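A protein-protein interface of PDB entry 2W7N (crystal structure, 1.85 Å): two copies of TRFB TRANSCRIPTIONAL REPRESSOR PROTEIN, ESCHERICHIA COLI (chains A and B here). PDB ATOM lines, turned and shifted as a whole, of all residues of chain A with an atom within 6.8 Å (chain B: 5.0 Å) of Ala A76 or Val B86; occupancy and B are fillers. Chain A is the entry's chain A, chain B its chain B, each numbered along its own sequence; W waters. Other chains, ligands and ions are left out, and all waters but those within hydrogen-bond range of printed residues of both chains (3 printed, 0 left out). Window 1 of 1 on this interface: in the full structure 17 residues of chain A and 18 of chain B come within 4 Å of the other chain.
The backbone carbonyl oxygen (O) of Ala A76 sits at hydrogen-bond distance from the backbone NH (N) of Val B74 (2.9 Å). O of Leu A78 lies within hydrogen-bond range of N of Ala B72, at 2.9 Å. The side-chain amide nitrogen (NE2) of Gln A82 sits close to the indole nitrogen (NE1) of Trp B89 (3.5 Å). The indole nitrogen of Trp A89 sits close to the side-chain amide nitrogen of Gln B82.
Among the printed residues, merely in contact across the chains: Thr A75 with Val B74 (3.2 Å), Val A77 with Ala B72 (3.4 Å), Ala A76 with Arg B73 (3.4 Å), Val A74 with Ala B83 (3.4 Å), Leu A78 with Val B74 (3.5 Å), Val A77 with Arg B73 (3.5 Å), Ala A76 with Ala B72 (3.6 Å), Val A86 with Val B86 (3.6 Å), Leu A78 with Trp B89 (3.7 Å), Thr A75 with Arg B73 (3.8 Å), Val A86 with Val B74 (3.8 Å), Thr A75 with Glu B90 (3.8 Å), Ala A76 with Val B86 (3.8 Å), Ala A76 with Glu B90 (3.8 Å), Val A74 with Leu B78 (3.9 Å), Val A74 with Arg B87 (3.9 Å), Val A74 with Val B74 (3.96 Å), Trp A89 with Trp B89 (3.97 Å), Trp A89 with Leu B78 (3.995 Å) and Trp A89 with Val B86 (3.997 Å).
Printed residues of chain B within 4 Å of Thr A75: Arg B73, Val B74 and Glu B90. Printed residues of chain B within 4 Å of Leu A78: Ala B72, Val B74 and Trp B89. Printed residues of chain B within 4 Å of Trp A89: Leu B78 (3.995 Å), Gln B82 (3.3 Å), Val B86 (3.997 Å) and Trp B89 (3.97 Å). Of the printed residues of chain A, Arg B73 touches Thr A75, Ala A76 and Val A77. Tyr B84 touches none of the printed residues of chain A. Of the printed residues of chain A, Val B86 touches Ala A76 (3.8 Å), Val A86 (3.6 Å) and Trp A89 (3.997 Å). Of the printed residues of chain A, Arg B87 touches Val A74. The nearest printed residue of chain A that does not touch Val B86 is Leu A78 (4.2 Å).
Of the 13 printed residues of chain B, 10 touch a printed residue of chain A. Among the printed residues, 24 pairs touch across the chains.
Val A74 touches Leu B78, and with the chains exchanged Leu A78 touches Val B74. Leu A78 touches Trp B89, and with the chains exchanged Trp A89 touches Leu B78. Val A86 touches Val B74, but with the chains exchanged Val A74 does not touch Val B86 (4.3 Å). Trp A89 touches its own counterpart, Trp B89. Of the 24 pairs that touch across the chains among the printed residues, 9 have their exchanged pair printed and touching as well.
Water W3 bridges OE1 of Gln A82 (2.5 Å) and O of Trp B89 (2.8 Å). Water W2 lies within hydrogen-bond range of the backbone carbonyl oxygen of Val A77 (2.7 Å) and the backbone carbonyl oxygen of Glu B90 (3.0 Å). Water W1 lies within hydrogen-bond range of OE2 of Glu B90 (2.8 Å) and N of Val A77 (2.9 Å).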
ATOM      1  N   VAL A  74      -4.564  -4.774  20.872  1.00  0.00           N
ATOM      2  CA  VAL A  74      -5.576  -5.336  19.980  1.00  0.00           C
ATOM      3  C   VAL A  74      -6.795  -4.446  20.008  1.00  0.00           C
ATOM      4  O   VAL A  74      -7.127  -3.885  21.046  1.00  0.00           O
ATOM      5  CB  VAL A  74      -6.004  -6.779  20.371  1.00  0.00           C
ATOM      6  CG1 VAL A  74      -4.937  -7.772  19.983  1.00  0.00           C
ATOM      7  CG2 VAL A  74      -6.328  -6.875  21.874  1.00  0.00           C
ATOM      8  N   THR A  75      -7.434  -4.298  18.853  1.00  0.00           N
ATOM      9  CA  THR A  75      -8.725  -3.633  18.753  1.00  0.00           C
ATOM     10  C   THR A  75      -9.683  -4.572  18.029  1.00  0.00           C
ATOM     11  O   THR A  75      -9.314  -5.202  17.037  1.00  0.00           O
ATOM     12  CB  THR A  75      -8.628  -2.290  18.000  1.00  0.00           C
ATOM     13  OG1 THR A  75      -7.637  -1.462  18.619  1.00  0.00           O
ATOM     14  CG2 THR A  75      -9.961  -1.554  18.025  1.00  0.00           C
ATOM     15  N   ALA A  76     -10.905  -4.681  18.540  1.00  0.00           N
ATOM     16  CA  ALA A  76     -11.880  -5.614  17.991  1.00  0.00           C
ATOM     17  C   ALA A  76     -13.289  -5.180  18.339  1.00  0.00           C
ATOM     18  O   ALA A  76     -13.517  -4.581  19.394  1.00  0.00           O
ATOM     19  CB  ALA A  76     -11.620  -7.033  18.533  1.00  0.00           C
ATOM     20  N   VAL A  77     -14.226  -5.482  17.445  1.00  0.00           N
ATOM     21  CA  VAL A  77     -15.648  -5.340  17.737  1.00  0.00           C
ATOM     22  C   VAL A  77     -16.112  -6.689  18.303  1.00  0.00           C
ATOM     23  O   VAL A  77     -15.961  -7.732  17.655  1.00  0.00           O
ATOM     24  CB  VAL A  77     -16.455  -4.916  16.488  1.00  0.00           C
ATOM     25  CG1 VAL A  77     -17.947  -5.000  16.757  1.00  0.00           C
ATOM     26  CG2 VAL A  77     -16.083  -3.497  16.074  1.00  0.00           C
ATOM     27  N   LEU A  78     -16.628  -6.663  19.527  1.00  0.00           N
ATOM     28  CA  LEU A  78     -16.972  -7.878  20.256  1.00  0.00           C
ATOM     29  C   LEU A  78     -18.383  -7.811  20.815  1.00  0.00           C
ATOM     30  O   LEU A  78     -18.876  -6.717  21.142  1.00  0.00           O
ATOM     31  CB  LEU A  78     -15.995  -8.088  21.418  1.00  0.00           C
ATOM     32  CG  LEU A  78     -14.529  -8.313  21.042  1.00  0.00           C
ATOM     33  CD1 LEU A  78     -13.625  -8.234  22.277  1.00  0.00           C
ATOM     34  CD2 LEU A  78     -14.377  -9.638  20.331  1.00  0.00           C
ATOM     35  N   GLN A  82     -17.961 -10.839  25.728  1.00  0.00           N
ATOM     36  CA  GLN A  82     -16.520 -10.855  25.430  1.00  0.00           C
ATOM     37  C   GLN A  82     -15.871  -9.500  25.691  1.00  0.00           C
ATOM     38  O   GLN A  82     -14.757  -9.426  26.227  1.00  0.00           O
ATOM     39  CB  GLN A  82     -16.281 -11.316  23.997  1.00  0.00           C
ATOM     40  CG  GLN A  82     -16.600 -12.806  23.832  1.00  0.00           C
ATOM     41  CD  GLN A  82     -16.612 -13.267  22.392  1.00  0.00           C
ATOM     42  OE1 GLN A  82     -16.507 -12.467  21.468  1.00  0.00           O
ATOM     43  NE2 GLN A  82     -16.719 -14.577  22.195  1.00  0.00           N
ATOM     44  N   VAL A  86     -12.646  -8.696  28.294  1.00  0.00           N
ATOM     45  CA  VAL A  86     -11.455  -7.923  27.942  1.00  0.00           C
ATOM     46  C   VAL A  86     -11.273  -6.740  28.895  1.00  0.00           C
ATOM     47  O   VAL A  86     -10.188  -6.529  29.416  1.00  0.00           O
ATOM     48  CB  VAL A  86     -11.488  -7.436  26.473  1.00  0.00           C
ATOM     49  CG1 VAL A  86     -10.354  -6.414  26.194  1.00  0.00           C
ATOM     50  CG2 VAL A  86     -11.395  -8.636  25.512  1.00  0.00           C
ATOM     51  N   TRP A  89     -10.079  -8.098  32.220  1.00  0.00           N
ATOM     52  CA  TRP A  89      -8.642  -8.416  32.168  1.00  0.00           C
ATOM     53  C   TRP A  89      -7.842  -7.138  32.433  1.00  0.00           C
ATOM     54  O   TRP A  89      -6.928  -7.129  33.254  1.00  0.00           O
ATOM     55  CB  TRP A  89      -8.237  -9.015  30.813  1.00  0.00           C
ATOM     56  CG  TRP A  89      -8.592 -10.455  30.598  1.00  0.00           C
ATOM     57  CD1 TRP A  89      -8.745 -11.410  31.551  1.00  0.00           C
ATOM     58  CD2 TRP A  89      -8.800 -11.112  29.337  1.00  0.00           C
ATOM     59  NE1 TRP A  89      -9.056 -12.614  30.976  1.00  0.00           N
ATOM     60  CE2 TRP A  89      -9.098 -12.460  29.617  1.00  0.00           C
ATOM     61  CE3 TRP A  89      -8.764 -10.687  28.000  1.00  0.00           C
ATOM     62  CZ2 TRP A  89      -9.350 -13.402  28.608  1.00  0.00           C
ATOM     63  CZ3 TRP A  89      -9.034 -11.607  27.005  1.00  0.00           C
ATOM     64  CH2 TRP A  89      -9.317 -12.961  27.315  1.00  0.00           C
ATOM     65  N   ALA B  72     -19.557  -3.876  20.803  1.00  0.00           N
ATOM     66  CA  ALA B  72     -18.783  -2.679  21.089  1.00  0.00           C
ATOM     67  C   ALA B  72     -17.356  -2.828  20.592  1.00  0.00           C
ATOM     68  O   ALA B  72     -16.796  -3.928  20.601  1.00  0.00           O
ATOM     69  CB  ALA B  72     -18.789  -2.385  22.585  1.00  0.00           C
ATOM     70  N   ARG B  73     -16.773  -1.719  20.150  1.00  0.00           N
ATOM     71  CA  ARG B  73     -15.369  -1.712  19.772  1.00  0.00           C
ATOM     72  C   ARG B  73     -14.549  -1.507  21.031  1.00  0.00           C
ATOM     73  O   ARG B  73     -14.718  -0.509  21.734  1.00  0.00           O
ATOM     74  CB  ARG B  73     -15.062  -0.615  18.749  1.00  0.00           C
ATOM     75  CG  ARG B  73     -13.576  -0.534  18.379  1.00  0.00           C
ATOM     76  CD  ARG B  73     -13.312   0.454  17.257  1.00  0.00           C
ATOM     77  NE  ARG B  73     -14.044   0.122  16.038  1.00  0.00           N
ATOM     78  CZ  ARG B  73     -13.705  -0.844  15.182  1.00  0.00           C
ATOM     79  NH1 ARG B  73     -12.627  -1.605  15.385  1.00  0.00           N
ATOM     80  NH2 ARG B  73     -14.459  -1.051  14.108  1.00  0.00           N
ATOM     81  N   VAL B  74     -13.666  -2.465  21.307  1.00  0.00           N
ATOM     82  CA  VAL B  74     -12.780  -2.423  22.463  1.00  0.00           C
ATOM     83  C   VAL B  74     -11.328  -2.410  21.980  1.00  0.00           C
ATOM     84  O   VAL B  74     -10.997  -3.047  20.977  1.00  0.00           O
ATOM     85  CB  VAL B  74     -13.009  -3.643  23.386  1.00  0.00           C
ATOM     86  CG1 VAL B  74     -12.632  -4.924  22.678  1.00  0.00           C
ATOM     87  CG2 VAL B  74     -12.203  -3.510  24.672  1.00  0.00           C
ATOM     88  N   LEU B  78      -2.738  -6.422  26.033  1.00  0.00           N
ATOM     89  CA  LEU B  78      -2.904  -7.704  26.706  1.00  0.00           C
ATOM     90  C   LEU B  78      -1.716  -8.616  26.462  1.00  0.00           C
ATOM     91  O   LEU B  78      -1.025  -8.472  25.454  1.00  0.00           O
ATOM     92  CB  LEU B  78      -4.150  -8.412  26.155  1.00  0.00           C
ATOM     93  CG  LEU B  78      -5.513  -7.747  26.334  1.00  0.00           C
ATOM     94  CD1 LEU B  78      -6.559  -8.449  25.453  1.00  0.00           C
ATOM     95  CD2 LEU B  78      -5.912  -7.774  27.810  1.00  0.00           C
ATOM     96  N   GLN B  82      -3.794 -13.762  25.316  1.00  0.00           N
ATOM     97  CA  GLN B  82      -5.119 -13.150  25.432  1.00  0.00           C
ATOM     98  C   GLN B  82      -5.479 -12.308  24.201  1.00  0.00           C
ATOM     99  O   GLN B  82      -6.630 -12.322  23.757  1.00  0.00           O
ATOM    100  CB  GLN B  82      -5.258 -12.373  26.748  1.00  0.00           C
ATOM    101  CG  GLN B  82      -5.437 -13.297  27.948  1.00  0.00           C
ATOM    102  CD  GLN B  82      -5.464 -12.572  29.294  1.00  0.00           C
ATOM    103  OE1 GLN B  82      -5.131 -11.391  29.385  1.00  0.00           O
ATOM    104  NE2 GLN B  82      -5.882 -13.285  30.344  1.00  0.00           N
ATOM    105  N   ALA B  83      -4.495 -11.616  23.624  1.00  0.00           N
ATOM    106  CA  ALA B  83      -4.681 -10.952  22.322  1.00  0.00           C
ATOM    107  C   ALA B  83      -5.077 -11.960  21.237  1.00  0.00           C
ATOM    108  O   ALA B  83      -5.929 -11.680  20.411  1.00  0.00           O
ATOM    109  CB  ALA B  83      -3.418 -10.172  21.917  1.00  0.00           C
ATOM    110  N   TYR B  84      -4.493 -13.151  21.284  1.00  0.00           N
ATOM    111  CA  TYR B  84      -4.851 -14.260  20.386  1.00  0.00           C
ATOM    112  C   TYR B  84      -6.318 -14.689  20.529  1.00  0.00           C
ATOM    113  O   TYR B  84      -7.039 -14.842  19.533  1.00  0.00           O
ATOM    114  CB  TYR B  84      -3.907 -15.434  20.657  1.00  0.00           C
ATOM    115  CG  TYR B  84      -4.334 -16.782  20.133  1.00  0.00           C
ATOM    116  CD1 TYR B  84      -4.299 -17.062  18.782  1.00  0.00           C
ATOM    117  CD2 TYR B  84      -4.741 -17.793  20.996  1.00  0.00           C
ATOM    118  CE1 TYR B  84      -4.676 -18.290  18.295  1.00  0.00           C
ATOM    119  CE2 TYR B  84      -5.112 -19.042  20.511  1.00  0.00           C
ATOM    120  CZ  TYR B  84      -5.073 -19.278  19.156  1.00  0.00           C
ATOM    121  OH  TYR B  84      -5.436 -20.503  18.633  1.00  0.00           O
ATOM    122  N   ILE B  85      -6.747 -14.881  21.773  1.00  0.00           N
ATOM    123  CA  ILE B  85      -8.133 -15.192  22.082  1.00  0.00           C
ATOM    124  C   ILE B  85      -9.088 -14.122  21.511  1.00  0.00           C
ATOM    125  O   ILE B  85     -10.118 -14.453  20.905  1.00  0.00           O
ATOM    126  CB  ILE B  85      -8.326 -15.353  23.622  1.00  0.00           C
ATOM    127  CG1 ILE B  85      -7.621 -16.627  24.118  1.00  0.00           C
ATOM    128  CG2 ILE B  85      -9.798 -15.424  23.992  1.00  0.00           C
ATOM    129  CD1 ILE B  85      -7.539 -16.737  25.642  1.00  0.00           C
ATOM    130  N   VAL B  86      -8.735 -12.856  21.682  1.00  0.00           N
ATOM    131  CA  VAL B  86      -9.542 -11.747  21.173  1.00  0.00           C
ATOM    132  C   VAL B  86      -9.602 -11.752  19.645  1.00  0.00           C
ATOM    133  O   VAL B  86     -10.676 -11.572  19.063  1.00  0.00           O
ATOM    134  CB  VAL B  86      -9.047 -10.386  21.703  1.00  0.00           C
ATOM    135  CG1 VAL B  86      -9.777  -9.207  21.005  1.00  0.00           C
ATOM    136  CG2 VAL B  86      -9.247 -10.318  23.228  1.00  0.00           C
ATOM    137  N   ARG B  87      -8.460 -11.978  19.001  1.00  0.00           N
ATOM    138  CA  ARG B  87      -8.425 -12.089  17.540  1.00  0.00           C
ATOM    139  C   ARG B  87      -9.348 -13.198  17.025  1.00  0.00           C
ATOM    140  O   ARG B  87     -10.020 -13.025  15.995  1.00  0.00           O
ATOM    141  CB  ARG B  87      -6.999 -12.327  17.048  1.00  0.00           C
ATOM    142  CG  ARG B  87      -6.061 -11.139  17.227  1.00  0.00           C
ATOM    143  CD  ARG B  87      -4.621 -11.549  16.984  1.00  0.00           C
ATOM    144  NE  ARG B  87      -3.646 -10.610  17.558  1.00  0.00           N
ATOM    145  CZ  ARG B  87      -2.542 -10.977  18.207  1.00  0.00           C
ATOM    146  NH1 ARG B  87      -2.261 -12.261  18.399  1.00  0.00           N
ATOM    147  NH2 ARG B  87      -1.720 -10.057  18.695  1.00  0.00           N
ATOM    148  N   LYS B  88      -9.386 -14.331  17.732  1.00  0.00           N
ATOM    149  CA  LYS B  88     -10.291 -15.430  17.386  1.00  0.00           C
ATOM    150  C   LYS B  88     -11.756 -15.043  17.583  1.00  0.00           C
ATOM    151  O   LYS B  88     -12.597 -15.322  16.735  1.00  0.00           O
ATOM    152  CB  LYS B  88      -9.983 -16.688  18.202  1.00  0.00           C
ATOM    153  CG  LYS B  88      -8.751 -17.462  17.756  1.00  0.00           C
ATOM    154  CD  LYS B  88      -8.956 -18.985  17.845  1.00  0.00           C
ATOM    155  CE  LYS B  88      -8.647 -19.567  19.222  1.00  0.00           C
ATOM    156  NZ  LYS B  88      -9.057 -18.702  20.348  1.00  0.00           N
ATOM    157  N   TRP B  89     -12.062 -14.420  18.714  1.00  0.00           N
ATOM    158  CA  TRP B  89     -13.408 -13.926  18.973  1.00  0.00           C
ATOM    159  C   TRP B  89     -13.874 -12.944  17.903  1.00  0.00           C
ATOM    160  O   TRP B  89     -15.051 -12.936  17.519  1.00  0.00           O
ATOM    161  CB  TRP B  89     -13.462 -13.224  20.317  1.00  0.00           C
ATOM    162  CG  TRP B  89     -13.433 -14.124  21.497  1.00  0.00           C
ATOM    163  CD1 TRP B  89     -13.666 -15.468  21.526  1.00  0.00           C
ATOM    164  CD2 TRP B  89     -13.212 -13.724  22.848  1.00  0.00           C
ATOM    165  NE1 TRP B  89     -13.574 -15.933  22.815  1.00  0.00           N
ATOM    166  CE2 TRP B  89     -13.297 -14.883  23.648  1.00  0.00           C
ATOM    167  CE3 TRP B  89     -12.915 -12.498  23.457  1.00  0.00           C
ATOM    168  CZ2 TRP B  89     -13.117 -14.853  25.031  1.00  0.00           C
ATOM    169  CZ3 TRP B  89     -12.735 -12.465  24.832  1.00  0.00           C
ATOM    170  CH2 TRP B  89     -12.839 -13.635  25.606  1.00  0.00           C
ATOM    171  N   GLU B  90     -12.951 -12.103  17.447  1.00  0.00           N
ATOM    172  CA  GLU B  90     -13.238 -11.109  16.421  1.00  0.00           C
ATOM    173  C   GLU B  90     -13.672 -11.803  15.126  1.00  0.00           C
ATOM    174  O   GLU B  90     -14.628 -11.376  14.482  1.00  0.00           O
ATOM    175  CB  GLU B  90     -12.012 -10.216  16.198  1.00  0.00           C
ATOM    176  CG  GLU B  90     -12.122  -9.218  15.051  1.00  0.00           C
ATOM    177  CD  GLU B  90     -10.877  -8.357  14.907  1.00  0.00           C
ATOM    178  OE1 GLU B  90      -9.872  -8.640  15.593  1.00  0.00           O
ATOM    179  OE2 GLU B  90     -10.896  -7.403  14.103  1.00  0.00           O
HETATM  180  O   HOH W   1     -13.373  -6.169  14.719  1.00  0.00           O
HETATM  181  O   HOH W   2     -15.682  -8.604  15.132  1.00  0.00           O
HETATM  182  O   HOH W   3     -17.237 -13.370  19.209  1.00  0.00           O
